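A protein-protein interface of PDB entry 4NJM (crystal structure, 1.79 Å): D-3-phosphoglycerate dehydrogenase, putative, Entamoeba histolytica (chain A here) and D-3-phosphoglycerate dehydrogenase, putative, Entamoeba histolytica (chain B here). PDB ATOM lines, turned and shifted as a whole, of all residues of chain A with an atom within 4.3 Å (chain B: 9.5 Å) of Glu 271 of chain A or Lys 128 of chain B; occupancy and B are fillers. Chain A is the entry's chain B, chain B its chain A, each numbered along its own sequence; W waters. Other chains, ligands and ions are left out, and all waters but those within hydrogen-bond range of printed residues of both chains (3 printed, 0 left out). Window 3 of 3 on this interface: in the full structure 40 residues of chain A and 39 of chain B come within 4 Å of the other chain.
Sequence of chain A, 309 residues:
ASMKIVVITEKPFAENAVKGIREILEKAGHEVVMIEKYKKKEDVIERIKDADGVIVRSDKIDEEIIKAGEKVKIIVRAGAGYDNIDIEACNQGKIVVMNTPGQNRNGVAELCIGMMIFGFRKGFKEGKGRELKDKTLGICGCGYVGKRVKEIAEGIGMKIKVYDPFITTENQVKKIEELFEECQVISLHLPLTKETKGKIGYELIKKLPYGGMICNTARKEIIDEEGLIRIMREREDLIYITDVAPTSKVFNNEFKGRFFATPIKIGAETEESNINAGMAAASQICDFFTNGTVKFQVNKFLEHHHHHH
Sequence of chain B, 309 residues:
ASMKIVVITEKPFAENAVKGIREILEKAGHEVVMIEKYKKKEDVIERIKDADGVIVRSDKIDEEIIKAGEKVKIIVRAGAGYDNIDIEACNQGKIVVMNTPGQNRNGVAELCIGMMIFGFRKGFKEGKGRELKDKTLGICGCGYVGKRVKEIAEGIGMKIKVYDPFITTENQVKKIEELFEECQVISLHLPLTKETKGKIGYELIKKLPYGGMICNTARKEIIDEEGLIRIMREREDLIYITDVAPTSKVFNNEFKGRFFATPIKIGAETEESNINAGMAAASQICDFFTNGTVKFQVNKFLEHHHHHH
The side-chain amino group (NZ) of Lys 128 of chain B sits at hydrogen-bond distance from the backbone carbonyl oxygen (O) of Pro 12 of chain A (2.6 Å).
The side-chain carboxylate (OE2) of Glu 131 of chain B sits at hydrogen-bond distance from the side-chain hydroxyl (OG1) of Thr 270 of chain A.
NZ of Lys 128 of chain B sits close to ND2 of Asn 274 of chain A, at 2.7 Å.
OE2 of Glu 272 of chain A is in salt-bridge range of NZ of Lys 135 of chain B, at 2.8 Å.
OE2 of Glu 269 of chain A lies within salt-bridge range of NZ of Lys 128 of chain B, 2.7 Å away.
The backbone NH (N) of Gly 129 of chain B lies within hydrogen-bond range of the backbone carbonyl oxygen (O) of Glu 269 of chain A, 2.8 Å away.
OG of Ser 273 of chain A is in hydrogen-bond range of OE2 of Glu 131 of chain B, 2.7 Å away.
O of Gly 129 of chain B lies within hydrogen-bond range of N of Glu 271 of chain A, at 3.1 Å.
The backbone NH (N) of Glu 131 of chain B sits at hydrogen-bond distance from the side-chain carboxylate (OE2) of Glu 272 of chain A (3.0 Å).
The side-chain amino group of Lys 135 of chain B sits at hydrogen-bond distance from the backbone carbonyl oxygen of Glu 131 of chain B, 2.9 Å away.
NH2 of Arg 57 of chain A is in hydrogen-bond range of OD1 of Asn 274 of chain A (3.5 Å).
The guanidinium group (NH2) of Arg 57 of chain A is in salt-bridge range of the side-chain carboxylate (OE2) of Glu 269 of chain A.
The backbone carbonyl oxygen of Pro 12 of chain A lies within hydrogen-bond range of the guanidinium group of Arg 57 of chain A.
ND2 of Asn 274 of chain A lies close to N of Ala 14 of chain A (2.8 Å).
The side-chain hydroxyl (OG1) of Thr 270 of chain A lies within hydrogen-bond range of the backbone NH (N) of Ser 273 of chain A, 3.0 Å away.
Among the printed residues, pairs that only touch across the chains: Phe 13 of chain A with Lys 128 of chain B (3.7 Å), Ala 14 of chain A with Lys 128 of chain B (3.6 Å), Arg 57 of chain A with Lys 128 of chain B (3.6 Å), Glu 269 of chain A with Gly 127 of chain B (3.6 Å), Thr 270 of chain A with Arg 121 of chain B (3.4 Å), Thr 270 of chain A with Gly 129 of chain B (3.2 Å), Glu 271 of chain A with Lys 128 of chain B (3.7 Å) and Glu 272 of chain A with Arg 130 of chain B (3.5 Å).
Of the printed residues of chain B, Ala 14 of chain A touches Lys 128 (3.6 Å).
Of the printed residues of chain B, Glu 269 of chain A touches Gly 127 (3.6 Å), Lys 128 (2.7 Å) and Gly 129 (2.8 Å).
Of chain B, only Arg 121, Gly 129 and Glu 131 come within 4 Å of Thr 270 of chain A.
Of chain B, only Lys 128 and Gly 129 come within 4 Å of Glu 271 of chain A.
Asn 274 of chain A touches one residue of chain B.
Lys 128 of chain B touches just these residues of chain A: Pro 12 (2.6 Å), Phe 13 (3.7 Å), Ala 14 (3.6 Å), Arg 57 (3.6 Å), Glu 269 (2.7 Å), Glu 271 (3.7 Å) and Asn 274 (2.7 Å).
Of the printed residues of chain A, Lys 135 of chain B touches Glu 272.
The nearest residue of chain B that does not touch Glu 271 of chain A is Arg 130 of chain B (4.5 Å).
The nearest printed residue of chain A that does not touch Lys 128 of chain B is Thr 270 of chain A (4.9 Å).
Printed residues of chain A that touch a printed residue of chain B: Pro 12, Phe 13, Ala 14, Arg 57, Glu 269, Thr 270, Glu 271, Glu 272, Ser 273 and Asn 274.
Of the 18 printed residues of chain B, 7 touch a printed residue of chain A.
Among the printed residues, 17 pairs touch across the chains.
Water W3 bridges NE of Arg 121 of chain B and O of Glu 269 of chain A.
Water W1 lies within hydrogen-bond range of OE1 of Glu 269 of chain A (2.8 Å), O of Pro 12 of chain A (2.8 Å) and NZ of Lys 128 of chain B (3.3 Å).
Water W2 bridges the backbone NH of Gly 127 of chain B and the side-chain carboxylate of Glu 269 of chain A.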
ATOM      1  N   PRO A  12       3.269  19.919   7.607  1.00  0.00           N
ATOM      2  CA  PRO A  12       3.836  18.579   7.805  1.00  0.00           C
ATOM      3  C   PRO A  12       4.532  18.359   9.152  1.00  0.00           C
ATOM      4  O   PRO A  12       5.039  19.312   9.765  1.00  0.00           O
ATOM      5  CB  PRO A  12       4.841  18.446   6.651  1.00  0.00           C
ATOM      6  CG  PRO A  12       4.372  19.425   5.623  1.00  0.00           C
ATOM      7  CD  PRO A  12       3.853  20.587   6.427  1.00  0.00           C
ATOM      8  N   PHE A  13       4.523  17.108   9.609  1.00  0.00           N
ATOM      9  CA  PHE A  13       5.306  16.689  10.754  1.00  0.00           C
ATOM     10  C   PHE A  13       6.787  16.747  10.405  1.00  0.00           C
ATOM     11  O   PHE A  13       7.152  16.666   9.228  1.00  0.00           O
ATOM     12  CB  PHE A  13       5.022  15.232  11.095  1.00  0.00           C
ATOM     13  CG  PHE A  13       3.694  14.987  11.723  1.00  0.00           C
ATOM     14  CD1 PHE A  13       3.406  15.473  12.995  1.00  0.00           C
ATOM     15  CD2 PHE A  13       2.745  14.219  11.061  1.00  0.00           C
ATOM     16  CE1 PHE A  13       2.177  15.212  13.588  1.00  0.00           C
ATOM     17  CE2 PHE A  13       1.517  13.953  11.651  1.00  0.00           C
ATOM     18  CZ  PHE A  13       1.235  14.457  12.910  1.00  0.00           C
ATOM     19  N   ALA A  14       7.624  16.826  11.439  1.00  0.00           N
ATOM     20  CA  ALA A  14       9.072  16.741  11.282  1.00  0.00           C
ATOM     21  C   ALA A  14       9.430  15.438  10.572  1.00  0.00           C
ATOM     22  O   ALA A  14       8.711  14.445  10.694  1.00  0.00           O
ATOM     23  CB  ALA A  14       9.754  16.807  12.639  1.00  0.00           C
ATOM     24  N   ARG A  57      -3.757  16.608  11.519  1.00  0.00           N
ATOM     25  CA  ARG A  57      -3.409  17.641  12.493  1.00  0.00           C
ATOM     26  C   ARG A  57      -4.571  18.632  12.611  1.00  0.00           C
ATOM     27  O   ARG A  57      -5.682  18.210  12.952  1.00  0.00           O
ATOM     28  CB  ARG A  57      -2.064  18.307  12.160  1.00  0.00           C
ATOM     29  CG  ARG A  57      -0.876  17.380  12.363  1.00  0.00           C
ATOM     30  CD  ARG A  57       0.439  18.080  12.045  1.00  0.00           C
ATOM     31  NE  ARG A  57       0.894  18.939  13.144  1.00  0.00           N
ATOM     32  CZ  ARG A  57       2.064  19.571  13.159  1.00  0.00           C
ATOM     33  NH1 ARG A  57       2.896  19.460  12.132  1.00  0.00           N
ATOM     34  NH2 ARG A  57       2.404  20.322  14.203  1.00  0.00           N
ATOM     35  N   GLU A 269       4.898  22.762  16.978  1.00  0.00           N
ATOM     36  CA  GLU A 269       5.920  22.649  15.932  1.00  0.00           C
ATOM     37  C   GLU A 269       7.324  22.479  16.514  1.00  0.00           C
ATOM     38  O   GLU A 269       8.186  23.350  16.362  1.00  0.00           O
ATOM     39  CB  GLU A 269       5.866  23.853  14.990  1.00  0.00           C
ATOM     40  CG  GLU A 269       4.687  23.818  14.034  1.00  0.00           C
ATOM     41  CD  GLU A 269       4.897  22.789  12.942  1.00  0.00           C
ATOM     42  OE1 GLU A 269       5.414  23.174  11.878  1.00  0.00           O
ATOM     43  OE2 GLU A 269       4.587  21.603  13.168  1.00  0.00           O
ATOM     44  N   THR A 270       7.535  21.359  17.193  1.00  0.00           N
ATOM     45  CA  THR A 270       8.855  20.990  17.688  1.00  0.00           C
ATOM     46  C   THR A 270       9.122  19.550  17.292  1.00  0.00           C
ATOM     47  O   THR A 270       8.184  18.784  17.068  1.00  0.00           O
ATOM     48  CB  THR A 270       8.963  21.110  19.216  1.00  0.00           C
ATOM     49  OG1 THR A 270       8.052  20.192  19.839  1.00  0.00           O
ATOM     50  CG2 THR A 270       8.635  22.538  19.669  1.00  0.00           C
ATOM     51  N   GLU A 271      10.401  19.192  17.202  1.00  0.00           N
ATOM     52  CA  GLU A 271      10.799  17.813  16.940  1.00  0.00           C
ATOM     53  C   GLU A 271      10.160  16.852  17.940  1.00  0.00           C
ATOM     54  O   GLU A 271       9.619  15.816  17.552  1.00  0.00           O
ATOM     55  CB  GLU A 271      12.324  17.690  17.009  1.00  0.00           C
ATOM     56  CG  GLU A 271      13.043  18.538  15.968  1.00  0.00           C
ATOM     57  CD  GLU A 271      12.893  17.991  14.555  1.00  0.00           C
ATOM     58  OE1 GLU A 271      12.694  16.761  14.416  1.00  0.00           O
ATOM     59  OE2 GLU A 271      12.986  18.791  13.590  1.00  0.00           O
ATOM     60  N   GLU A 272      10.202  17.230  19.218  1.00  0.00           N
ATOM     61  CA  GLU A 272       9.787  16.363  20.315  1.00  0.00           C
ATOM     62  C   GLU A 272       8.280  16.138  20.330  1.00  0.00           C
ATOM     63  O   GLU A 272       7.811  15.011  20.542  1.00  0.00           O
ATOM     64  CB  GLU A 272      10.224  16.948  21.665  1.00  0.00           C
ATOM     65  CG  GLU A 272      11.727  17.157  21.839  1.00  0.00           C
ATOM     66  CD  GLU A 272      12.220  18.508  21.354  1.00  0.00           C
ATOM     67  OE1 GLU A 272      11.535  19.174  20.553  1.00  0.00           O
ATOM     68  OE2 GLU A 272      13.325  18.910  21.770  1.00  0.00           O
ATOM     69  N   SER A 273       7.523  17.212  20.130  1.00  0.00           N
ATOM     70  CA  SER A 273       6.058  17.106  20.148  1.00  0.00           C
ATOM     71  C   SER A 273       5.520  16.407  18.902  1.00  0.00           C
ATOM     72  O   SER A 273       4.563  15.630  18.998  1.00  0.00           O
ATOM     73  CB  SER A 273       5.400  18.474  20.378  1.00  0.00           C
ATOM     74  OG  SER A 273       5.541  18.832  21.749  1.00  0.00           O
ATOM     75  N   ASN A 274       6.138  16.660  17.748  1.00  0.00           N
ATOM     76  CA  ASN A 274       5.776  15.949  16.509  1.00  0.00           C
ATOM     77  C   ASN A 274       5.974  14.439  16.652  1.00  0.00           C
ATOM     78  O   ASN A 274       5.098  13.651  16.270  1.00  0.00           O
ATOM     79  CB  ASN A 274       6.574  16.446  15.296  1.00  0.00           C
ATOM     80  CG  ASN A 274       6.066  17.766  14.730  1.00  0.00           C
ATOM     81  OD1 ASN A 274       5.105  18.377  15.225  1.00  0.00           O
ATOM     82  ND2 ASN A 274       6.721  18.216  13.685  1.00  0.00           N
ATOM     83  N   ILE A 275       7.128  14.043  17.189  1.00  0.00           N
ATOM     84  CA  ILE A 275       7.424  12.628  17.463  1.00  0.00           C
ATOM     85  C   ILE A 275       6.375  12.018  18.406  1.00  0.00           C
ATOM     86  O   ILE A 275       5.794  10.963  18.106  1.00  0.00           O
ATOM     87  CB  ILE A 275       8.867  12.446  18.001  1.00  0.00           C
ATOM     88  CG1 ILE A 275       9.865  12.553  16.842  1.00  0.00           C
ATOM     89  CG2 ILE A 275       9.021  11.112  18.728  1.00  0.00           C
ATOM     90  CD1 ILE A 275      11.317  12.748  17.259  1.00  0.00           C
ATOM     91  N   PHE B 118      12.833  31.520  23.048  1.00  0.00           N
ATOM     92  CA  PHE B 118      12.852  32.249  21.777  1.00  0.00           C
ATOM     93  C   PHE B 118      13.880  31.657  20.802  1.00  0.00           C
ATOM     94  O   PHE B 118      13.553  31.392  19.643  1.00  0.00           O
ATOM     95  CB  PHE B 118      13.192  33.704  22.088  1.00  0.00           C
ATOM     96  CG  PHE B 118      12.997  34.665  20.944  1.00  0.00           C
ATOM     97  CD1 PHE B 118      11.724  35.082  20.569  1.00  0.00           C
ATOM     98  CD2 PHE B 118      14.097  35.213  20.304  1.00  0.00           C
ATOM     99  CE1 PHE B 118      11.549  36.002  19.551  1.00  0.00           C
ATOM    100  CE2 PHE B 118      13.928  36.141  19.285  1.00  0.00           C
ATOM    101  CZ  PHE B 118      12.656  36.530  18.907  1.00  0.00           C
ATOM    102  N   GLY B 119      15.103  31.451  21.289  1.00  0.00           N
ATOM    103  CA  GLY B 119      16.200  30.882  20.490  1.00  0.00           C
ATOM    104  C   GLY B 119      15.919  29.477  19.973  1.00  0.00           C
ATOM    105  O   GLY B 119      16.260  29.151  18.838  1.00  0.00           O
ATOM    106  N   PHE B 120      15.277  28.653  20.800  1.00  0.00           N
ATOM    107  CA  PHE B 120      14.953  27.267  20.442  1.00  0.00           C
ATOM    108  C   PHE B 120      13.698  27.178  19.575  1.00  0.00           C
ATOM    109  O   PHE B 120      13.433  26.136  18.972  1.00  0.00           O
ATOM    110  CB  PHE B 120      14.753  26.432  21.723  1.00  0.00           C
ATOM    111  CG  PHE B 120      15.827  25.400  21.983  1.00  0.00           C
ATOM    112  CD1 PHE B 120      17.118  25.544  21.482  1.00  0.00           C
ATOM    113  CD2 PHE B 120      15.543  24.291  22.778  1.00  0.00           C
ATOM    114  CE1 PHE B 120      18.097  24.592  21.753  1.00  0.00           C
ATOM    115  CE2 PHE B 120      16.516  23.335  23.049  1.00  0.00           C
ATOM    116  CZ  PHE B 120      17.795  23.488  22.533  1.00  0.00           C
ATOM    117  N   ARG B 121      12.932  28.269  19.515  1.00  0.00           N
ATOM    118  CA  ARG B 121      11.654  28.283  18.793  1.00  0.00           C
ATOM    119  C   ARG B 121      11.654  29.268  17.618  1.00  0.00           C
ATOM    120  O   ARG B 121      10.655  29.945  17.353  1.00  0.00           O
ATOM    121  CB  ARG B 121      10.489  28.563  19.760  1.00  0.00           C
ATOM    122  CG  ARG B 121      10.355  27.546  20.886  1.00  0.00           C
ATOM    123  CD  ARG B 121      10.047  26.145  20.372  1.00  0.00           C
ATOM    124  NE  ARG B 121       8.633  25.967  20.024  1.00  0.00           N
ATOM    125  CZ  ARG B 121       7.681  25.581  20.875  1.00  0.00           C
ATOM    126  NH1 ARG B 121       6.436  25.425  20.435  1.00  0.00           N
ATOM    127  NH2 ARG B 121       7.963  25.338  22.155  1.00  0.00           N
ATOM    128  N   LYS B 122      12.789  29.323  16.916  1.00  0.00           N
ATOM    129  CA  LYS B 122      12.944  30.071  15.651  1.00  0.00           C
ATOM    130  C   LYS B 122      12.601  31.558  15.774  1.00  0.00           C
ATOM    131  O   LYS B 122      12.167  32.190  14.813  1.00  0.00           O
ATOM    132  CB  LYS B 122      12.112  29.435  14.514  1.00  0.00           C
ATOM    133  CG  LYS B 122      12.205  27.915  14.375  1.00  0.00           C
ATOM    134  CD  LYS B 122      13.575  27.433  13.938  1.00  0.00           C
ATOM    135  CE  LYS B 122      13.765  27.519  12.433  1.00  0.00           C
ATOM    136  NZ  LYS B 122      15.033  26.831  12.075  1.00  0.00           N
ATOM    137  N   GLY B 123      12.788  32.127  16.955  1.00  0.00           N
ATOM    138  CA  GLY B 123      12.415  33.526  17.160  1.00  0.00           C
ATOM    139  C   GLY B 123      10.935  33.784  16.939  1.00  0.00           C
ATOM    140  O   GLY B 123      10.542  34.869  16.483  1.00  0.00           O
ATOM    141  N   LYS B 125       9.097  32.427  14.749  1.00  0.00           N
ATOM    142  CA  LYS B 125       8.792  32.346  13.318  1.00  0.00           C
ATOM    143  C   LYS B 125       8.396  30.910  12.967  1.00  0.00           C
ATOM    144  O   LYS B 125       8.465  30.013  13.810  1.00  0.00           O
ATOM    145  CB  LYS B 125      10.004  32.766  12.477  1.00  0.00           C
ATOM    146  CG  LYS B 125      10.466  34.196  12.701  1.00  0.00           C
ATOM    147  CD  LYS B 125      11.573  34.571  11.723  1.00  0.00           C
ATOM    148  CE  LYS B 125      12.056  35.993  11.952  1.00  0.00           C
ATOM    149  NZ  LYS B 125      10.976  37.003  11.758  1.00  0.00           N
ATOM    150  N   GLU B 126       7.968  30.714  11.723  1.00  0.00           N
ATOM    151  CA  GLU B 126       7.624  29.404  11.174  1.00  0.00           C
ATOM    152  C   GLU B 126       8.804  28.423  11.215  1.00  0.00           C
ATOM    153  O   GLU B 126       9.964  28.836  11.180  1.00  0.00           O
ATOM    154  CB  GLU B 126       7.194  29.609   9.717  1.00  0.00           C
ATOM    155  CG  GLU B 126       6.201  28.610   9.163  1.00  0.00           C
ATOM    156  CD  GLU B 126       5.813  28.916   7.721  1.00  0.00           C
ATOM    157  OE1 GLU B 126       6.640  29.495   6.981  1.00  0.00           O
ATOM    158  OE2 GLU B 126       4.680  28.576   7.321  1.00  0.00           O
ATOM    159  N   GLY B 127       8.500  27.128  11.291  1.00  0.00           N
ATOM    160  CA  GLY B 127       9.528  26.089  11.233  1.00  0.00           C
ATOM    161  C   GLY B 127       9.569  25.197  12.459  1.00  0.00           C
ATOM    162  O   GLY B 127       8.828  25.409  13.431  1.00  0.00           O
ATOM    163  N   LYS B 128      10.435  24.189  12.418  1.00  0.00           N
ATOM    164  CA  LYS B 128      10.513  23.222  13.504  1.00  0.00           C
ATOM    165  C   LYS B 128      11.448  23.706  14.600  1.00  0.00           C
ATOM    166  O   LYS B 128      12.618  23.991  14.339  1.00  0.00           O
ATOM    167  CB  LYS B 128      10.986  21.858  12.990  1.00  0.00           C
ATOM    168  CG  LYS B 128      10.092  21.247  11.933  1.00  0.00           C
ATOM    169  CD  LYS B 128       8.687  20.987  12.451  1.00  0.00           C
ATOM    170  CE  LYS B 128       7.803  20.523  11.310  1.00  0.00           C
ATOM    171  NZ  LYS B 128       6.451  20.177  11.807  1.00  0.00           N
ATOM    172  N   GLY B 129      10.922  23.811  15.817  1.00  0.00           N
ATOM    173  CA  GLY B 129      11.718  24.202  16.973  1.00  0.00           C
ATOM    174  C   GLY B 129      12.113  23.017  17.824  1.00  0.00           C
ATOM    175  O   GLY B 129      11.965  21.867  17.407  1.00  0.00           O
ATOM    176  N   ARG B 130      12.641  23.304  19.011  1.00  0.00           N
ATOM    177  CA  ARG B 130      12.972  22.279  19.992  1.00  0.00           C
ATOM    178  C   ARG B 130      12.530  22.732  21.368  1.00  0.00           C
ATOM    179  O   ARG B 130      12.209  23.903  21.566  1.00  0.00           O
ATOM    180  CB  ARG B 130      14.481  22.020  20.014  1.00  0.00           C
ATOM    181  CG  ARG B 130      15.023  21.420  18.728  1.00  0.00           C
ATOM    182  CD  ARG B 130      16.512  21.121  18.832  1.00  0.00           C
ATOM    183  NE  ARG B 130      17.333  22.316  18.990  1.00  0.00           N
ATOM    184  CZ  ARG B 130      17.819  23.044  17.985  1.00  0.00           C
ATOM    185  NH1 ARG B 130      17.552  22.723  16.724  1.00  0.00           N
ATOM    186  NH2 ARG B 130      18.561  24.105  18.244  1.00  0.00           N
ATOM    187  N   GLU B 131      12.549  21.798  22.317  1.00  0.00           N
ATOM    188  CA  GLU B 131      12.107  22.044  23.685  1.00  0.00           C
ATOM    189  C   GLU B 131      13.282  21.987  24.652  1.00  0.00           C
ATOM    190  O   GLU B 131      14.204  21.175  24.488  1.00  0.00           O
ATOM    191  CB  GLU B 131      11.028  21.028  24.079  1.00  0.00           C
ATOM    192  CG  GLU B 131       9.868  21.026  23.088  1.00  0.00           C
ATOM    193  CD  GLU B 131       8.856  19.922  23.311  1.00  0.00           C
ATOM    194  OE1 GLU B 131       9.000  19.134  24.267  1.00  0.00           O
ATOM    195  OE2 GLU B 131       7.902  19.850  22.516  1.00  0.00           O
ATOM    196  N   LYS B 135      16.649  18.548  28.195  1.00  0.00           N
ATOM    197  CA  LYS B 135      17.967  18.939  27.708  1.00  0.00           C
ATOM    198  C   LYS B 135      18.850  19.278  28.893  1.00  0.00           C
ATOM    199  O   LYS B 135      18.357  19.536  29.993  1.00  0.00           O
ATOM    200  CB  LYS B 135      17.895  20.137  26.754  1.00  0.00           C
ATOM    201  CG  LYS B 135      16.910  19.990  25.601  1.00  0.00           C
ATOM    202  CD  LYS B 135      17.150  18.753  24.752  1.00  0.00           C
ATOM    203  CE  LYS B 135      16.171  18.677  23.587  1.00  0.00           C
ATOM    204  NZ  LYS B 135      14.789  18.384  24.067  1.00  0.00           N
ATOM    205  N   GLN B 184      24.043  20.878  26.259  1.00  0.00           N
ATOM    206  CA  GLN B 184      23.526  21.314  24.961  1.00  0.00           C
ATOM    207  C   GLN B 184      23.171  22.803  24.942  1.00  0.00           C
ATOM    208  O   GLN B 184      23.245  23.451  23.898  1.00  0.00           O
ATOM    209  CB  GLN B 184      22.317  20.489  24.542  1.00  0.00           C
ATOM    210  CG  GLN B 184      21.911  20.701  23.087  1.00  0.00           C
ATOM    211  CD  GLN B 184      20.610  20.012  22.734  1.00  0.00           C
ATOM    212  OE1 GLN B 184      20.114  19.174  23.488  1.00  0.00           O
ATOM    213  NE2 GLN B 184      20.051  20.356  21.577  1.00  0.00           N
ATOM    214  N   TYR B 210      25.387  18.516  19.248  1.00  0.00           N
ATOM    215  CA  TYR B 210      24.575  18.952  18.120  1.00  0.00           C
ATOM    216  C   TYR B 210      23.335  19.711  18.589  1.00  0.00           C
ATOM    217  O   TYR B 210      22.710  19.343  19.590  1.00  0.00           O
ATOM    218  CB  TYR B 210      24.161  17.778  17.238  1.00  0.00           C
ATOM    219  CG  TYR B 210      23.617  18.223  15.898  1.00  0.00           C
ATOM    220  CD1 TYR B 210      24.473  18.494  14.834  1.00  0.00           C
ATOM    221  CD2 TYR B 210      22.244  18.388  15.697  1.00  0.00           C
ATOM    222  CE1 TYR B 210      23.981  18.904  13.606  1.00  0.00           C
ATOM    223  CE2 TYR B 210      21.742  18.805  14.472  1.00  0.00           C
ATOM    224  CZ  TYR B 210      22.617  19.059  13.431  1.00  0.00           C
ATOM    225  OH  TYR B 210      22.129  19.470  12.217  1.00  0.00           O
ATOM    226  N   ILE B 239      23.241  27.918  17.736  1.00  0.00           N
ATOM    227  CA  ILE B 239      22.424  29.122  17.928  1.00  0.00           C
ATOM    228  C   ILE B 239      23.097  30.028  18.951  1.00  0.00           C
ATOM    229  O   ILE B 239      23.540  29.559  19.990  1.00  0.00           O
ATOM    230  CB  ILE B 239      21.010  28.765  18.441  1.00  0.00           C
ATOM    231  CG1 ILE B 239      20.253  27.900  17.423  1.00  0.00           C
ATOM    232  CG2 ILE B 239      20.217  30.025  18.772  1.00  0.00           C
ATOM    233  CD1 ILE B 239      19.013  27.246  18.005  1.00  0.00           C
ATOM    234  N   GLY B 257      18.229  33.499  11.502  1.00  0.00           N
ATOM    235  CA  GLY B 257      17.579  32.217  11.749  1.00  0.00           C
ATOM    236  C   GLY B 257      18.186  31.458  12.908  1.00  0.00           C
ATOM    237  O   GLY B 257      17.544  30.574  13.475  1.00  0.00           O
HETATM  238  O   HOH W   1       5.468  22.077   9.327  1.00  0.00           O
HETATM  239  O   HOH W   2       5.937  25.935  11.281  1.00  0.00           O
HETATM  240  O   HOH W   3       8.622  26.099  17.265  1.00  0.00           O
